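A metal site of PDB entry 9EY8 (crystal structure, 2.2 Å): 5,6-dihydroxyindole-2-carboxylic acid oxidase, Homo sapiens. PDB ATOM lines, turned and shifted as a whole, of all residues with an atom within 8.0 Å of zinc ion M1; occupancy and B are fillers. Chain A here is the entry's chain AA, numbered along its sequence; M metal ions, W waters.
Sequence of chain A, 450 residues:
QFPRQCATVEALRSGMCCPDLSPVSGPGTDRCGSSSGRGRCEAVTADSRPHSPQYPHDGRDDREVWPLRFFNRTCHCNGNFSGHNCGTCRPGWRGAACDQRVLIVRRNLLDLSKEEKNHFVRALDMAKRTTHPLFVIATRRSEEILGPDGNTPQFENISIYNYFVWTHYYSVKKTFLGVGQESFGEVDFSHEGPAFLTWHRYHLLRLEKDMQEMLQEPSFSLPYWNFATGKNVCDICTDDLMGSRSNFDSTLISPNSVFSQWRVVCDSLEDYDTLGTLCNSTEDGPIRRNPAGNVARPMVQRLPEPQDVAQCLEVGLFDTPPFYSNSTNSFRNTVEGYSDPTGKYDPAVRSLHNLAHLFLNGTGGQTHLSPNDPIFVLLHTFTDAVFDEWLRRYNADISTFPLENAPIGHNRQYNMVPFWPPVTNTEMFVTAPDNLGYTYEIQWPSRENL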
ATOM      1  N   HIS A 168      -9.384 -26.444  -5.247  1.00  0.00           N
ATOM      2  CA  HIS A 168     -10.354 -25.462  -5.708  1.00  0.00           C
ATOM      3  C   HIS A 168     -10.899 -24.630  -4.555  1.00  0.00           C
ATOM      4  O   HIS A 168     -10.885 -23.389  -4.621  1.00  0.00           O
ATOM      5  CB  HIS A 168     -11.478 -26.193  -6.430  1.00  0.00           C
ATOM      6  CG  HIS A 168     -12.319 -25.287  -7.271  1.00  0.00           C
ATOM      7  ND1 HIS A 168     -13.524 -24.762  -6.831  1.00  0.00           N
ATOM      8  CD2 HIS A 168     -12.100 -24.759  -8.489  1.00  0.00           C
ATOM      9  CE1 HIS A 168     -14.013 -23.975  -7.760  1.00  0.00           C
ATOM     10  NE2 HIS A 168     -13.172 -23.954  -8.782  1.00  0.00           N
ATOM     11  N   SER A 190      -8.399 -18.009  -8.435  1.00  0.00           N
ATOM     12  CA  SER A 190      -8.671 -18.810  -9.626  1.00  0.00           C
ATOM     13  C   SER A 190      -9.851 -18.327 -10.447  1.00  0.00           C
ATOM     14  O   SER A 190     -10.167 -18.974 -11.461  1.00  0.00           O
ATOM     15  CB  SER A 190      -8.897 -20.272  -9.237  1.00  0.00           C
ATOM     16  OG  SER A 190      -9.889 -20.331  -8.218  1.00  0.00           O
ATOM     17  N   HIS A 191     -10.514 -17.238 -10.052  1.00  0.00           N
ATOM     18  CA  HIS A 191     -11.653 -16.677 -10.771  1.00  0.00           C
ATOM     19  C   HIS A 191     -11.555 -15.161 -10.791  1.00  0.00           C
ATOM     20  O   HIS A 191     -10.844 -14.559  -9.982  1.00  0.00           O
ATOM     21  CB  HIS A 191     -13.002 -17.051 -10.102  1.00  0.00           C
ATOM     22  CG  HIS A 191     -13.201 -18.502  -9.969  1.00  0.00           C
ATOM     23  ND1 HIS A 191     -12.536 -19.279  -9.045  1.00  0.00           N
ATOM     24  CD2 HIS A 191     -13.952 -19.365 -10.705  1.00  0.00           C
ATOM     25  CE1 HIS A 191     -12.890 -20.541  -9.186  1.00  0.00           C
ATOM     26  NE2 HIS A 191     -13.756 -20.613 -10.180  1.00  0.00           N
ATOM     27  N   PHE A 196      -8.021 -17.308 -14.531  1.00  0.00           N
ATOM     28  CA  PHE A 196      -9.149 -18.239 -14.505  1.00  0.00           C
ATOM     29  C   PHE A 196      -8.942 -19.413 -15.468  1.00  0.00           C
ATOM     30  O   PHE A 196      -9.160 -20.586 -15.108  1.00  0.00           O
ATOM     31  CB  PHE A 196     -10.456 -17.535 -14.843  1.00  0.00           C
ATOM     32  CG  PHE A 196     -11.552 -18.457 -15.226  1.00  0.00           C
ATOM     33  CD1 PHE A 196     -12.250 -19.181 -14.252  1.00  0.00           C
ATOM     34  CD2 PHE A 196     -11.918 -18.613 -16.554  1.00  0.00           C
ATOM     35  CE1 PHE A 196     -13.278 -20.032 -14.580  1.00  0.00           C
ATOM     36  CE2 PHE A 196     -12.928 -19.481 -16.926  1.00  0.00           C
ATOM     37  CZ  PHE A 196     -13.624 -20.199 -15.929  1.00  0.00           C
ATOM     38  N   HIS A 200      -7.628 -23.366 -14.205  1.00  0.00           N
ATOM     39  CA  HIS A 200      -8.503 -24.500 -14.395  1.00  0.00           C
ATOM     40  C   HIS A 200      -7.926 -25.500 -15.393  1.00  0.00           C
ATOM     41  O   HIS A 200      -8.243 -26.694 -15.310  1.00  0.00           O
ATOM     42  CB  HIS A 200      -9.882 -24.025 -14.857  1.00  0.00           C
ATOM     43  CG  HIS A 200     -10.709 -23.480 -13.743  1.00  0.00           C
ATOM     44  ND1 HIS A 200     -10.551 -22.210 -13.239  1.00  0.00           N
ATOM     45  CD2 HIS A 200     -11.684 -24.066 -13.008  1.00  0.00           C
ATOM     46  CE1 HIS A 200     -11.404 -22.021 -12.258  1.00  0.00           C
ATOM     47  NE2 HIS A 200     -12.123 -23.124 -12.108  1.00  0.00           N
ATOM     48  N   HIS A 203      -5.580 -27.613 -13.183  1.00  0.00           N
ATOM     49  CA  HIS A 203      -6.507 -28.391 -12.362  1.00  0.00           C
ATOM     50  C   HIS A 203      -6.924 -29.712 -13.036  1.00  0.00           C
ATOM     51  O   HIS A 203      -6.837 -30.799 -12.440  1.00  0.00           O
ATOM     52  CB  HIS A 203      -7.739 -27.505 -12.111  1.00  0.00           C
ATOM     53  CG  HIS A 203      -8.589 -27.943 -10.975  1.00  0.00           C
ATOM     54  ND1 HIS A 203      -9.955 -27.753 -10.965  1.00  0.00           N
ATOM     55  CD2 HIS A 203      -8.280 -28.493  -9.775  1.00  0.00           C
ATOM     56  CE1 HIS A 203     -10.449 -28.193  -9.821  1.00  0.00           C
ATOM     57  NE2 HIS A 203      -9.460 -28.653  -9.079  1.00  0.00           N
ATOM     58  N   GLU A 336     -15.464 -16.922 -19.219  1.00  0.00           N
ATOM     59  CA  GLU A 336     -15.763 -17.164 -17.812  1.00  0.00           C
ATOM     60  C   GLU A 336     -17.239 -16.877 -17.531  1.00  0.00           C
ATOM     61  O   GLU A 336     -17.904 -17.634 -16.807  1.00  0.00           O
ATOM     62  CB  GLU A 336     -14.836 -16.344 -16.901  1.00  0.00           C
ATOM     63  CG  GLU A 336     -14.952 -16.756 -15.402  1.00  0.00           C
ATOM     64  CD  GLU A 336     -14.057 -15.949 -14.433  1.00  0.00           C
ATOM     65  OE1 GLU A 336     -13.204 -15.161 -14.893  1.00  0.00           O
ATOM     66  OE2 GLU A 336     -14.222 -16.119 -13.187  1.00  0.00           O
ATOM     67  N   HIS A 353     -19.512 -20.168 -19.246  1.00  0.00           N
ATOM     68  CA  HIS A 353     -19.115 -21.049 -18.147  1.00  0.00           C
ATOM     69  C   HIS A 353     -19.901 -20.757 -16.856  1.00  0.00           C
ATOM     70  O   HIS A 353     -20.351 -21.686 -16.166  1.00  0.00           O
ATOM     71  CB  HIS A 353     -17.607 -20.940 -17.898  1.00  0.00           C
ATOM     72  CG  HIS A 353     -17.217 -21.037 -16.456  1.00  0.00           C
ATOM     73  ND1 HIS A 353     -17.244 -19.955 -15.611  1.00  0.00           N
ATOM     74  CD2 HIS A 353     -16.824 -22.098 -15.700  1.00  0.00           C
ATOM     75  CE1 HIS A 353     -16.864 -20.333 -14.408  1.00  0.00           C
ATOM     76  NE2 HIS A 353     -16.601 -21.616 -14.441  1.00  0.00           N
ATOM     77  N   ASN A 354     -20.055 -19.479 -16.499  1.00  0.00           N
ATOM     78  CA  ASN A 354     -20.829 -19.163 -15.296  1.00  0.00           C
ATOM     79  C   ASN A 354     -22.266 -19.679 -15.408  1.00  0.00           C
ATOM     80  O   ASN A 354     -22.796 -20.283 -14.463  1.00  0.00           O
ATOM     81  CB  ASN A 354     -20.832 -17.656 -15.036  1.00  0.00           C
ATOM     82  CG  ASN A 354     -19.540 -17.126 -14.420  1.00  0.00           C
ATOM     83  OD1 ASN A 354     -18.739 -17.875 -13.862  1.00  0.00           O
ATOM     84  ND2 ASN A 354     -19.349 -15.804 -14.485  1.00  0.00           N
ATOM     85  N   ALA A 356     -23.478 -22.142 -17.196  1.00  0.00           N
ATOM     86  CA  ALA A 356     -23.528 -23.594 -17.075  1.00  0.00           C
ATOM     87  C   ALA A 356     -23.503 -24.033 -15.601  1.00  0.00           C
ATOM     88  O   ALA A 356     -24.184 -24.990 -15.226  1.00  0.00           O
ATOM     89  CB  ALA A 356     -22.369 -24.222 -17.864  1.00  0.00           C
ATOM     90  N   HIS A 357     -22.724 -23.350 -14.756  1.00  0.00           N
ATOM     91  CA  HIS A 357     -22.757 -23.654 -13.324  1.00  0.00           C
ATOM     92  C   HIS A 357     -24.131 -23.383 -12.715  1.00  0.00           C
ATOM     93  O   HIS A 357     -24.663 -24.207 -11.967  1.00  0.00           O
ATOM     94  CB  HIS A 357     -21.702 -22.834 -12.567  1.00  0.00           C
ATOM     95  CG  HIS A 357     -20.356 -23.446 -12.583  1.00  0.00           C
ATOM     96  ND1 HIS A 357     -20.037 -24.576 -11.860  1.00  0.00           N
ATOM     97  CD2 HIS A 357     -19.226 -23.101 -13.259  1.00  0.00           C
ATOM     98  CE1 HIS A 357     -18.779 -24.907 -12.085  1.00  0.00           C
ATOM     99  NE2 HIS A 357     -18.267 -24.033 -12.929  1.00  0.00           N
ATOM    100  N   GLY A 364     -23.169 -27.833  -7.738  1.00  0.00           N
ATOM    101  CA  GLY A 364     -22.336 -27.436  -8.870  1.00  0.00           C
ATOM    102  C   GLY A 364     -22.393 -25.966  -9.217  1.00  0.00           C
ATOM    103  O   GLY A 364     -21.632 -25.531 -10.084  1.00  0.00           O
ATOM    104  N   THR A 367     -19.447 -21.616  -5.638  1.00  0.00           N
ATOM    105  CA  THR A 367     -18.048 -21.526  -6.026  1.00  0.00           C
ATOM    106  C   THR A 367     -17.156 -22.376  -5.128  1.00  0.00           C
ATOM    107  O   THR A 367     -16.280 -23.100  -5.612  1.00  0.00           O
ATOM    108  CB  THR A 367     -17.580 -20.064  -6.008  1.00  0.00           C
ATOM    109  OG1 THR A 367     -18.530 -19.236  -6.686  1.00  0.00           O
ATOM    110  CG2 THR A 367     -16.209 -19.922  -6.683  1.00  0.00           C
ATOM    111  N   SER A 370     -18.307 -26.332  -5.973  1.00  0.00           N
ATOM    112  CA  SER A 370     -18.809 -26.861  -7.244  1.00  0.00           C
ATOM    113  C   SER A 370     -18.109 -28.112  -7.774  1.00  0.00           C
ATOM    114  O   SER A 370     -18.798 -28.900  -8.448  1.00  0.00           O
ATOM    115  CB  SER A 370     -18.793 -25.755  -8.323  1.00  0.00           C
ATOM    116  OG  SER A 370     -17.484 -25.302  -8.567  1.00  0.00           O
ATOM    117  N   PRO A 371     -16.798 -28.353  -7.569  1.00  0.00           N
ATOM    118  CA  PRO A 371     -16.198 -29.628  -8.019  1.00  0.00           C
ATOM    119  C   PRO A 371     -16.795 -30.868  -7.371  1.00  0.00           C
ATOM    120  O   PRO A 371     -16.607 -31.960  -7.913  1.00  0.00           O
ATOM    121  CB  PRO A 371     -14.712 -29.489  -7.644  1.00  0.00           C
ATOM    122  CG  PRO A 371     -14.486 -28.010  -7.584  1.00  0.00           C
ATOM    123  CD  PRO A 371     -15.755 -27.479  -6.986  1.00  0.00           C
ATOM    124  N   PHE A 376     -18.633 -31.009 -12.913  1.00  0.00           N
ATOM    125  CA  PHE A 376     -17.590 -29.975 -12.949  1.00  0.00           C
ATOM    126  C   PHE A 376     -16.466 -30.331 -13.924  1.00  0.00           C
ATOM    127  O   PHE A 376     -16.034 -29.484 -14.714  1.00  0.00           O
ATOM    128  CB  PHE A 376     -17.025 -29.764 -11.525  1.00  0.00           C
ATOM    129  CG  PHE A 376     -15.966 -28.668 -11.421  1.00  0.00           C
ATOM    130  CD1 PHE A 376     -14.649 -28.911 -11.764  1.00  0.00           C
ATOM    131  CD2 PHE A 376     -16.317 -27.396 -10.981  1.00  0.00           C
ATOM    132  CE1 PHE A 376     -13.687 -27.911 -11.689  1.00  0.00           C
ATOM    133  CE2 PHE A 376     -15.376 -26.385 -10.885  1.00  0.00           C
ATOM    134  CZ  PHE A 376     -14.054 -26.641 -11.230  1.00  0.00           C
ATOM    135  N   LEU A 379     -17.734 -29.949 -17.484  1.00  0.00           N
ATOM    136  CA  LEU A 379     -17.991 -28.548 -17.762  1.00  0.00           C
ATOM    137  C   LEU A 379     -16.687 -27.805 -18.030  1.00  0.00           C
ATOM    138  O   LEU A 379     -16.629 -26.910 -18.881  1.00  0.00           O
ATOM    139  CB  LEU A 379     -18.772 -27.934 -16.590  1.00  0.00           C
ATOM    140  CG  LEU A 379     -19.326 -26.509 -16.571  1.00  0.00           C
ATOM    141  CD1 LEU A 379     -20.421 -26.363 -15.493  1.00  0.00           C
ATOM    142  CD2 LEU A 379     -18.217 -25.425 -16.381  1.00  0.00           C
ATOM    143  N   HIS A 380     -15.599 -28.205 -17.340  1.00  0.00           N
ATOM    144  CA  HIS A 380     -14.333 -27.502 -17.483  1.00  0.00           C
ATOM    145  C   HIS A 380     -13.424 -28.053 -18.562  1.00  0.00           C
ATOM    146  O   HIS A 380     -12.576 -27.288 -19.049  1.00  0.00           O
ATOM    147  CB  HIS A 380     -13.587 -27.479 -16.153  1.00  0.00           C
ATOM    148  CG  HIS A 380     -13.890 -26.256 -15.379  1.00  0.00           C
ATOM    149  ND1 HIS A 380     -13.463 -25.010 -15.806  1.00  0.00           N
ATOM    150  CD2 HIS A 380     -14.698 -26.041 -14.312  1.00  0.00           C
ATOM    151  CE1 HIS A 380     -13.952 -24.088 -14.983  1.00  0.00           C
ATOM    152  NE2 HIS A 380     -14.674 -24.700 -14.058  1.00  0.00           N
ATOM    153  N   THR A 383     -14.842 -26.011 -21.359  1.00  0.00           N
ATOM    154  CA  THR A 383     -14.310 -24.658 -21.236  1.00  0.00           C
ATOM    155  C   THR A 383     -12.840 -24.620 -21.644  1.00  0.00           C
ATOM    156  O   THR A 383     -12.402 -23.676 -22.311  1.00  0.00           O
ATOM    157  CB  THR A 383     -14.477 -24.157 -19.792  1.00  0.00           C
ATOM    158  OG1 THR A 383     -15.870 -24.096 -19.461  1.00  0.00           O
ATOM    159  CG2 THR A 383     -13.856 -22.741 -19.597  1.00  0.00           C
HETATM  160 ZN    ZN M   1     -16.169 -23.380 -13.145  1.00  0.00          ZN
HETATM  161 ZN    ZN M   2     -13.675 -22.738 -10.593  1.00  0.00          ZN
HETATM  162  O   HOH W   1     -15.522 -22.919 -11.410  1.00  0.00           O
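A ring nitrogen (ND1) of His 357 is in hydrogen-bond range of the backbone carbonyl oxygen of Gly 364 (2.6 Å). A ring nitrogen (ND1) of His 353 sits at hydrogen-bond distance from the side-chain amide oxygen (OD1) of Asn 354 (3.1 Å). The backbone carbonyl oxygen (O) of Glu 336 is in hydrogen-bond range of a ring nitrogen (ND1) of His 353.
Phe 376 touches zinc ion M1. Within 4 Å of zinc ion M1: His 353, His 357, Phe 376 and His 380. The nearest printed residue that does not touch zinc ion M1 is His 200 (4.2 Å).
Water W1 is bound to zinc ion M1, at 1.9 Å. Zinc ion M1 is bound by NE2 of His 380. Zinc ion M1 is bound by a ring nitrogen (NE2) of His 357. A ring nitrogen (NE2) of His 353 binds zinc ion M1 (2.2 Å). Zinc ion M1 has four donor atoms within binding distance.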
